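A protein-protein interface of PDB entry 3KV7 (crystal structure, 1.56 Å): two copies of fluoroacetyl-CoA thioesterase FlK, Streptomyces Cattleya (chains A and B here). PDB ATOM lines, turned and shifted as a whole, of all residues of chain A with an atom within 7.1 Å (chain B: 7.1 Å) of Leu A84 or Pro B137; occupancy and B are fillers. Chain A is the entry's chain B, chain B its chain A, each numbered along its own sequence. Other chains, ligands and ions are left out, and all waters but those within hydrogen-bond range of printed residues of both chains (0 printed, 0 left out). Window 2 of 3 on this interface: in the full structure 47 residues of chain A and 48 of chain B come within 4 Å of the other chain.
The side-chain amino group (NZ) of Lys B135 is in hydrogen-bond range of the backbone carbonyl oxygen (O) of Ala A79, 2.8 Å away. The side-chain amino group (NZ) of Lys B135 is in salt-bridge range of the side-chain carboxylate (OD2) of Asp A108, 2.8 Å away. OD2 of Asp A111 is in salt-bridge range of NZ of Lys B135 (2.7 Å).
The backbone carbonyl oxygen (O) of Val A17 lies within hydrogen-bond range of the backbone NH (N) of Gly A83, 2.8 Å away. OD2 of Asp A108 lies within hydrogen-bond range of OG1 of Thr A80, at 2.7 Å. OD1 of Asp A108 is in hydrogen-bond range of N of Val A110 (2.9 Å). The backbone carbonyl oxygen (O) of Val B132 sits at hydrogen-bond distance from the side-chain hydroxyl (OG1) of Thr B136, at 2.8 Å. The side-chain carboxylate of Asp A108 is in hydrogen-bond range of the backbone NH of Asp A111. The backbone NH (N) of Val A17 sits at hydrogen-bond distance from the backbone carbonyl oxygen (O) of Leu A84 (2.9 Å).
Pro A81 touches Val B132 (CB to CG1, 3.8 Å). Pro A81 touches Lys B135. Pro A81 touches Thr B136. Pro B137 touches Pro A82 (CD to O, 3.9 Å). CG of Pro B137 touches C of Gly A83, at 3.8 Å. Leu A84 touches Lys B135 (CD1 to O, 3.5 Å). Leu A84 touches Pro B137 (CD2 to CG, 3.8 Å). CB of Val A110 touches CE of Lys B135, at 3.96 Å.
Leu A84 touches just these residues of chain B: Lys B135 and Pro B137. Pro B137 touches just these residues of chain A: Pro A82, Gly A83 and Leu A84. Gly A83 touches just one residue of chain B: Pro B137. Printed residues of chain A within 4 Å of Thr B136: Pro A81 (3.4 Å). Printed residues of chain B within 4 Å of Asp A108: Lys B135. Of the printed residues of chain B, Val A110 touches Lys B135 (3.96 Å). Printed residues of chain A within 4 Å of Val B132: Pro A81. Of the printed residues of chain B, Ala A79 touches Lys B135. Thr A80 touches none of the printed residues of chain B. The nearest residue of chain B that does not touch Leu A84 is Thr B136 (5.6 Å). The nearest residue of chain A that does not touch Pro B137 is Pro A81 (4.6 Å).
Hydrophobic or aromatic side chains of chain A within 4 Å of the printed part of chain B: Pro A81, Leu A84 and Val A110. Hydrophobic or aromatic side chains of chain B within 4 Å of the printed part of chain A: Val B132 and Pro B137.
No position is printed for both chains.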
ATOM      1  N   PHE A  15      -5.219 -32.369 -17.573  1.00  0.00           N
ATOM      2  CA  PHE A  15      -5.233 -30.912 -17.627  1.00  0.00           C
ATOM      3  C   PHE A  15      -5.010 -30.351 -16.271  1.00  0.00           C
ATOM      4  O   PHE A  15      -5.825 -30.523 -15.336  1.00  0.00           O
ATOM      5  CB  PHE A  15      -6.618 -30.420 -18.180  1.00  0.00           C
ATOM      6  CG  PHE A  15      -6.749 -28.914 -18.244  1.00  0.00           C
ATOM      7  CD1 PHE A  15      -6.030 -28.215 -19.234  1.00  0.00           C
ATOM      8  CD2 PHE A  15      -7.582 -28.234 -17.346  1.00  0.00           C
ATOM      9  CE1 PHE A  15      -6.234 -26.764 -19.290  1.00  0.00           C
ATOM     10  CE2 PHE A  15      -7.757 -26.848 -17.372  1.00  0.00           C
ATOM     11  CZ  PHE A  15      -7.057 -26.112 -18.368  1.00  0.00           C
ATOM     12  N   VAL A  16      -3.875 -29.618 -16.107  1.00  0.00           N
ATOM     13  CA  VAL A  16      -3.645 -28.932 -14.812  1.00  0.00           C
ATOM     14  C   VAL A  16      -4.561 -27.699 -14.730  1.00  0.00           C
ATOM     15  O   VAL A  16      -4.511 -26.829 -15.595  1.00  0.00           O
ATOM     16  CB  VAL A  16      -2.124 -28.499 -14.679  1.00  0.00           C
ATOM     17  CG1 VAL A  16      -1.908 -27.704 -13.364  1.00  0.00           C
ATOM     18  CG2 VAL A  16      -1.228 -29.741 -14.692  1.00  0.00           C
ATOM     19  N   VAL A  17      -5.361 -27.603 -13.630  1.00  0.00           N
ATOM     20  CA  VAL A  17      -6.355 -26.497 -13.606  1.00  0.00           C
ATOM     21  C   VAL A  17      -5.605 -25.189 -13.210  1.00  0.00           C
ATOM     22  O   VAL A  17      -5.029 -25.133 -12.157  1.00  0.00           O
ATOM     23  CB  VAL A  17      -7.377 -26.821 -12.513  1.00  0.00           C
ATOM     24  CG1 VAL A  17      -8.424 -25.643 -12.346  1.00  0.00           C
ATOM     25  CG2 VAL A  17      -8.180 -28.135 -12.857  1.00  0.00           C
ATOM     26  N   PRO A  18      -5.660 -24.222 -14.111  1.00  0.00           N
ATOM     27  CA  PRO A  18      -5.014 -22.912 -13.805  1.00  0.00           C
ATOM     28  C   PRO A  18      -6.039 -22.033 -13.013  1.00  0.00           C
ATOM     29  O   PRO A  18      -7.253 -22.336 -12.924  1.00  0.00           O
ATOM     30  CB  PRO A  18      -4.796 -22.287 -15.165  1.00  0.00           C
ATOM     31  CG  PRO A  18      -5.876 -22.851 -16.068  1.00  0.00           C
ATOM     32  CD  PRO A  18      -6.285 -24.226 -15.432  1.00  0.00           C
ATOM     33  N   ALA A  79     -15.049 -30.871  -5.358  1.00  0.00           N
ATOM     34  CA  ALA A  79     -14.548 -29.595  -5.843  1.00  0.00           C
ATOM     35  C   ALA A  79     -13.013 -29.605  -5.995  1.00  0.00           C
ATOM     36  O   ALA A  79     -12.319 -30.273  -5.231  1.00  0.00           O
ATOM     37  CB  ALA A  79     -14.900 -28.472  -4.839  1.00  0.00           C
ATOM     38  N   THR A  80     -12.550 -28.820  -6.985  1.00  0.00           N
ATOM     39  CA  THR A  80     -11.139 -28.888  -7.342  1.00  0.00           C
ATOM     40  C   THR A  80     -10.560 -27.470  -7.417  1.00  0.00           C
ATOM     41  O   THR A  80     -10.942 -26.686  -8.208  1.00  0.00           O
ATOM     42  CB  THR A  80     -10.984 -29.516  -8.774  1.00  0.00           C
ATOM     43  OG1 THR A  80     -11.538 -30.824  -8.826  1.00  0.00           O
ATOM     44  CG2 THR A  80      -9.507 -29.624  -9.227  1.00  0.00           C
ATOM     45  N   PRO A  81      -9.551 -27.188  -6.524  1.00  0.00           N
ATOM     46  CA  PRO A  81      -8.820 -25.911  -6.609  1.00  0.00           C
ATOM     47  C   PRO A  81      -7.838 -25.897  -7.750  1.00  0.00           C
ATOM     48  O   PRO A  81      -7.381 -26.973  -8.186  1.00  0.00           O
ATOM     49  CB  PRO A  81      -8.081 -25.915  -5.246  1.00  0.00           C
ATOM     50  CG  PRO A  81      -7.776 -27.359  -4.950  1.00  0.00           C
ATOM     51  CD  PRO A  81      -9.059 -28.096  -5.502  1.00  0.00           C
ATOM     52  N   PRO A  82      -7.474 -24.698  -8.192  1.00  0.00           N
ATOM     53  CA  PRO A  82      -6.332 -24.593  -9.164  1.00  0.00           C
ATOM     54  C   PRO A  82      -5.087 -25.337  -8.646  1.00  0.00           C
ATOM     55  O   PRO A  82      -4.769 -25.407  -7.476  1.00  0.00           O
ATOM     56  CB  PRO A  82      -6.075 -23.107  -9.242  1.00  0.00           C
ATOM     57  CG  PRO A  82      -7.431 -22.443  -8.841  1.00  0.00           C
ATOM     58  CD  PRO A  82      -7.964 -23.368  -7.753  1.00  0.00           C
ATOM     59  N   GLY A  83      -4.410 -25.968  -9.587  1.00  0.00           N
ATOM     60  CA  GLY A  83      -3.117 -26.578  -9.337  1.00  0.00           C
ATOM     61  C   GLY A  83      -3.180 -28.093  -9.370  1.00  0.00           C
ATOM     62  O   GLY A  83      -2.136 -28.767  -9.593  1.00  0.00           O
ATOM     63  N   LEU A  84      -4.351 -28.691  -9.101  1.00  0.00           N
ATOM     64  CA  LEU A  84      -4.499 -30.141  -9.320  1.00  0.00           C
ATOM     65  C   LEU A  84      -4.649 -30.489 -10.807  1.00  0.00           C
ATOM     66  O   LEU A  84      -5.069 -29.634 -11.606  1.00  0.00           O
ATOM     67  CB  LEU A  84      -5.761 -30.718  -8.568  1.00  0.00           C
ATOM     68  CG  LEU A  84      -5.629 -30.652  -7.061  1.00  0.00           C
ATOM     69  CD1 LEU A  84      -6.822 -31.208  -6.394  1.00  0.00           C
ATOM     70  CD2 LEU A  84      -4.423 -31.367  -6.507  1.00  0.00           C
ATOM     71  N   THR A  85      -4.332 -31.748 -11.147  1.00  0.00           N
ATOM     72  CA  THR A  85      -4.552 -32.210 -12.547  1.00  0.00           C
ATOM     73  C   THR A  85      -5.904 -32.914 -12.581  1.00  0.00           C
ATOM     74  O   THR A  85      -6.103 -33.930 -11.863  1.00  0.00           O
ATOM     75  CB  THR A  85      -3.476 -33.234 -12.903  1.00  0.00           C
ATOM     76  OG1 THR A  85      -2.177 -32.553 -12.772  1.00  0.00           O
ATOM     77  CG2 THR A  85      -3.575 -33.697 -14.335  1.00  0.00           C
ATOM     78  N   VAL A  86      -6.763 -32.441 -13.477  1.00  0.00           N
ATOM     79  CA  VAL A  86      -8.016 -33.159 -13.750  1.00  0.00           C
ATOM     80  C   VAL A  86      -7.751 -34.070 -14.955  1.00  0.00           C
ATOM     81  O   VAL A  86      -7.253 -33.624 -16.064  1.00  0.00           O
ATOM     82  CB  VAL A  86      -9.115 -32.194 -14.136  1.00  0.00           C
ATOM     83  CG1 VAL A  86     -10.415 -33.024 -14.523  1.00  0.00           C
ATOM     84  CG2 VAL A  86      -9.504 -31.375 -12.906  1.00  0.00           C
ATOM     85  N   ASP A 108      -9.494 -35.686  -9.988  1.00  0.00           N
ATOM     86  CA  ASP A 108      -8.475 -34.598  -9.914  1.00  0.00           C
ATOM     87  C   ASP A 108      -7.205 -35.050  -9.158  1.00  0.00           C
ATOM     88  O   ASP A 108      -6.459 -34.205  -8.632  1.00  0.00           O
ATOM     89  CB  ASP A 108      -9.049 -33.325  -9.250  1.00  0.00           C
ATOM     90  CG  ASP A 108      -9.568 -33.574  -7.825  1.00  0.00           C
ATOM     91  OD1 ASP A 108      -9.241 -34.601  -7.174  1.00  0.00           O
ATOM     92  OD2 ASP A 108     -10.278 -32.661  -7.296  1.00  0.00           O
ATOM     93  N   GLY A 109      -7.015 -36.355  -9.132  1.00  0.00           N
ATOM     94  CA  GLY A 109      -5.842 -36.909  -8.405  1.00  0.00           C
ATOM     95  C   GLY A 109      -6.130 -37.168  -6.921  1.00  0.00           C
ATOM     96  O   GLY A 109      -5.424 -37.976  -6.257  1.00  0.00           O
ATOM     97  N   VAL A 110      -7.190 -36.570  -6.391  1.00  0.00           N
ATOM     98  CA  VAL A 110      -7.568 -36.720  -4.968  1.00  0.00           C
ATOM     99  C   VAL A 110      -8.887 -37.427  -4.923  1.00  0.00           C
ATOM    100  O   VAL A 110      -9.010 -38.539  -4.335  1.00  0.00           O
ATOM    101  CB  VAL A 110      -7.564 -35.361  -4.271  1.00  0.00           C
ATOM    102  CG1 VAL A 110      -8.056 -35.556  -2.770  1.00  0.00           C
ATOM    103  CG2 VAL A 110      -6.138 -34.765  -4.286  1.00  0.00           C
ATOM    104  N   ASP A 111      -9.880 -36.871  -5.649  1.00  0.00           N
ATOM    105  CA  ASP A 111     -11.195 -37.419  -5.646  1.00  0.00           C
ATOM    106  C   ASP A 111     -11.720 -37.619  -7.084  1.00  0.00           C
ATOM    107  O   ASP A 111     -11.308 -36.922  -7.998  1.00  0.00           O
ATOM    108  CB  ASP A 111     -12.165 -36.400  -5.066  1.00  0.00           C
ATOM    109  CG  ASP A 111     -11.912 -36.085  -3.604  1.00  0.00           C
ATOM    110  OD1 ASP A 111     -11.821 -37.078  -2.801  1.00  0.00           O
ATOM    111  OD2 ASP A 111     -11.756 -34.866  -3.228  1.00  0.00           O
ATOM    112  N   VAL B 132     -11.487 -27.335   0.869  1.00  0.00           N
ATOM    113  CA  VAL B 132     -10.817 -27.036  -0.435  1.00  0.00           C
ATOM    114  C   VAL B 132      -9.325 -26.815  -0.175  1.00  0.00           C
ATOM    115  O   VAL B 132      -8.481 -27.354  -0.873  1.00  0.00           O
ATOM    116  CB  VAL B 132     -11.441 -25.889  -1.221  1.00  0.00           C
ATOM    117  CG1 VAL B 132     -10.597 -25.526  -2.460  1.00  0.00           C
ATOM    118  CG2 VAL B 132     -12.889 -26.312  -1.662  1.00  0.00           C
ATOM    119  N   ARG B 133      -9.031 -26.016   0.858  1.00  0.00           N
ATOM    120  CA  ARG B 133      -7.600 -25.804   1.257  1.00  0.00           C
ATOM    121  C   ARG B 133      -6.837 -27.062   1.540  1.00  0.00           C
ATOM    122  O   ARG B 133      -5.644 -27.152   1.191  1.00  0.00           O
ATOM    123  CB  ARG B 133      -7.514 -24.837   2.449  1.00  0.00           C
ATOM    124  CG  ARG B 133      -7.927 -23.451   2.021  1.00  0.00           C
ATOM    125  CD  ARG B 133      -7.539 -22.365   3.013  1.00  0.00           C
ATOM    126  NE  ARG B 133      -8.624 -21.405   3.059  1.00  0.00           N
ATOM    127  CZ  ARG B 133      -9.537 -21.383   4.028  1.00  0.00           C
ATOM    128  NH1 ARG B 133     -10.526 -20.485   3.992  1.00  0.00           N
ATOM    129  NH2 ARG B 133      -9.422 -22.238   5.030  1.00  0.00           N
ATOM    130  N   GLN B 134      -7.460 -28.061   2.133  1.00  0.00           N
ATOM    131  CA  GLN B 134      -6.708 -29.251   2.369  1.00  0.00           C
ATOM    132  C   GLN B 134      -6.334 -30.123   1.200  1.00  0.00           C
ATOM    133  O   GLN B 134      -5.466 -30.974   1.358  1.00  0.00           O
ATOM    134  CB  GLN B 134      -7.194 -30.070   3.530  1.00  0.00           C
ATOM    135  CG  GLN B 134      -8.560 -30.437   3.565  1.00  0.00           C
ATOM    136  CD  GLN B 134      -8.913 -30.824   4.970  1.00  0.00           C
ATOM    137  OE1 GLN B 134      -8.055 -30.733   5.859  1.00  0.00           O
ATOM    138  NE2 GLN B 134     -10.175 -31.254   5.197  1.00  0.00           N
ATOM    139  N   LYS B 135      -6.946 -29.875   0.037  1.00  0.00           N
ATOM    140  CA  LYS B 135      -6.562 -30.599  -1.188  1.00  0.00           C
ATOM    141  C   LYS B 135      -5.902 -29.619  -2.187  1.00  0.00           C
ATOM    142  O   LYS B 135      -5.683 -29.995  -3.337  1.00  0.00           O
ATOM    143  CB  LYS B 135      -7.733 -31.438  -1.783  1.00  0.00           C
ATOM    144  CG  LYS B 135      -8.936 -30.638  -2.078  1.00  0.00           C
ATOM    145  CD  LYS B 135     -10.090 -31.548  -2.658  1.00  0.00           C
ATOM    146  CE  LYS B 135      -9.794 -32.095  -4.081  1.00  0.00           C
ATOM    147  NZ  LYS B 135     -11.083 -32.707  -4.626  1.00  0.00           N
ATOM    148  N   THR B 136      -5.549 -28.404  -1.727  1.00  0.00           N
ATOM    149  CA  THR B 136      -4.847 -27.414  -2.530  1.00  0.00           C
ATOM    150  C   THR B 136      -3.332 -27.667  -2.424  1.00  0.00           C
ATOM    151  O   THR B 136      -2.811 -27.747  -1.280  1.00  0.00           O
ATOM    152  CB  THR B 136      -5.138 -25.989  -2.101  1.00  0.00           C
ATOM    153  OG1 THR B 136      -6.566 -25.788  -2.130  1.00  0.00           O
ATOM    154  CG2 THR B 136      -4.438 -24.960  -3.014  1.00  0.00           C
ATOM    155  N   PRO B 137      -2.648 -27.827  -3.600  1.00  0.00           N
ATOM    156  CA  PRO B 137      -1.177 -28.033  -3.523  1.00  0.00           C
ATOM    157  C   PRO B 137      -0.463 -26.845  -2.878  1.00  0.00           C
ATOM    158  O   PRO B 137      -0.832 -25.672  -3.071  1.00  0.00           O
ATOM    159  CB  PRO B 137      -0.722 -28.196  -5.007  1.00  0.00           C
ATOM    160  CG  PRO B 137      -1.946 -28.542  -5.782  1.00  0.00           C
ATOM    161  CD  PRO B 137      -3.165 -27.924  -4.985  1.00  0.00           C
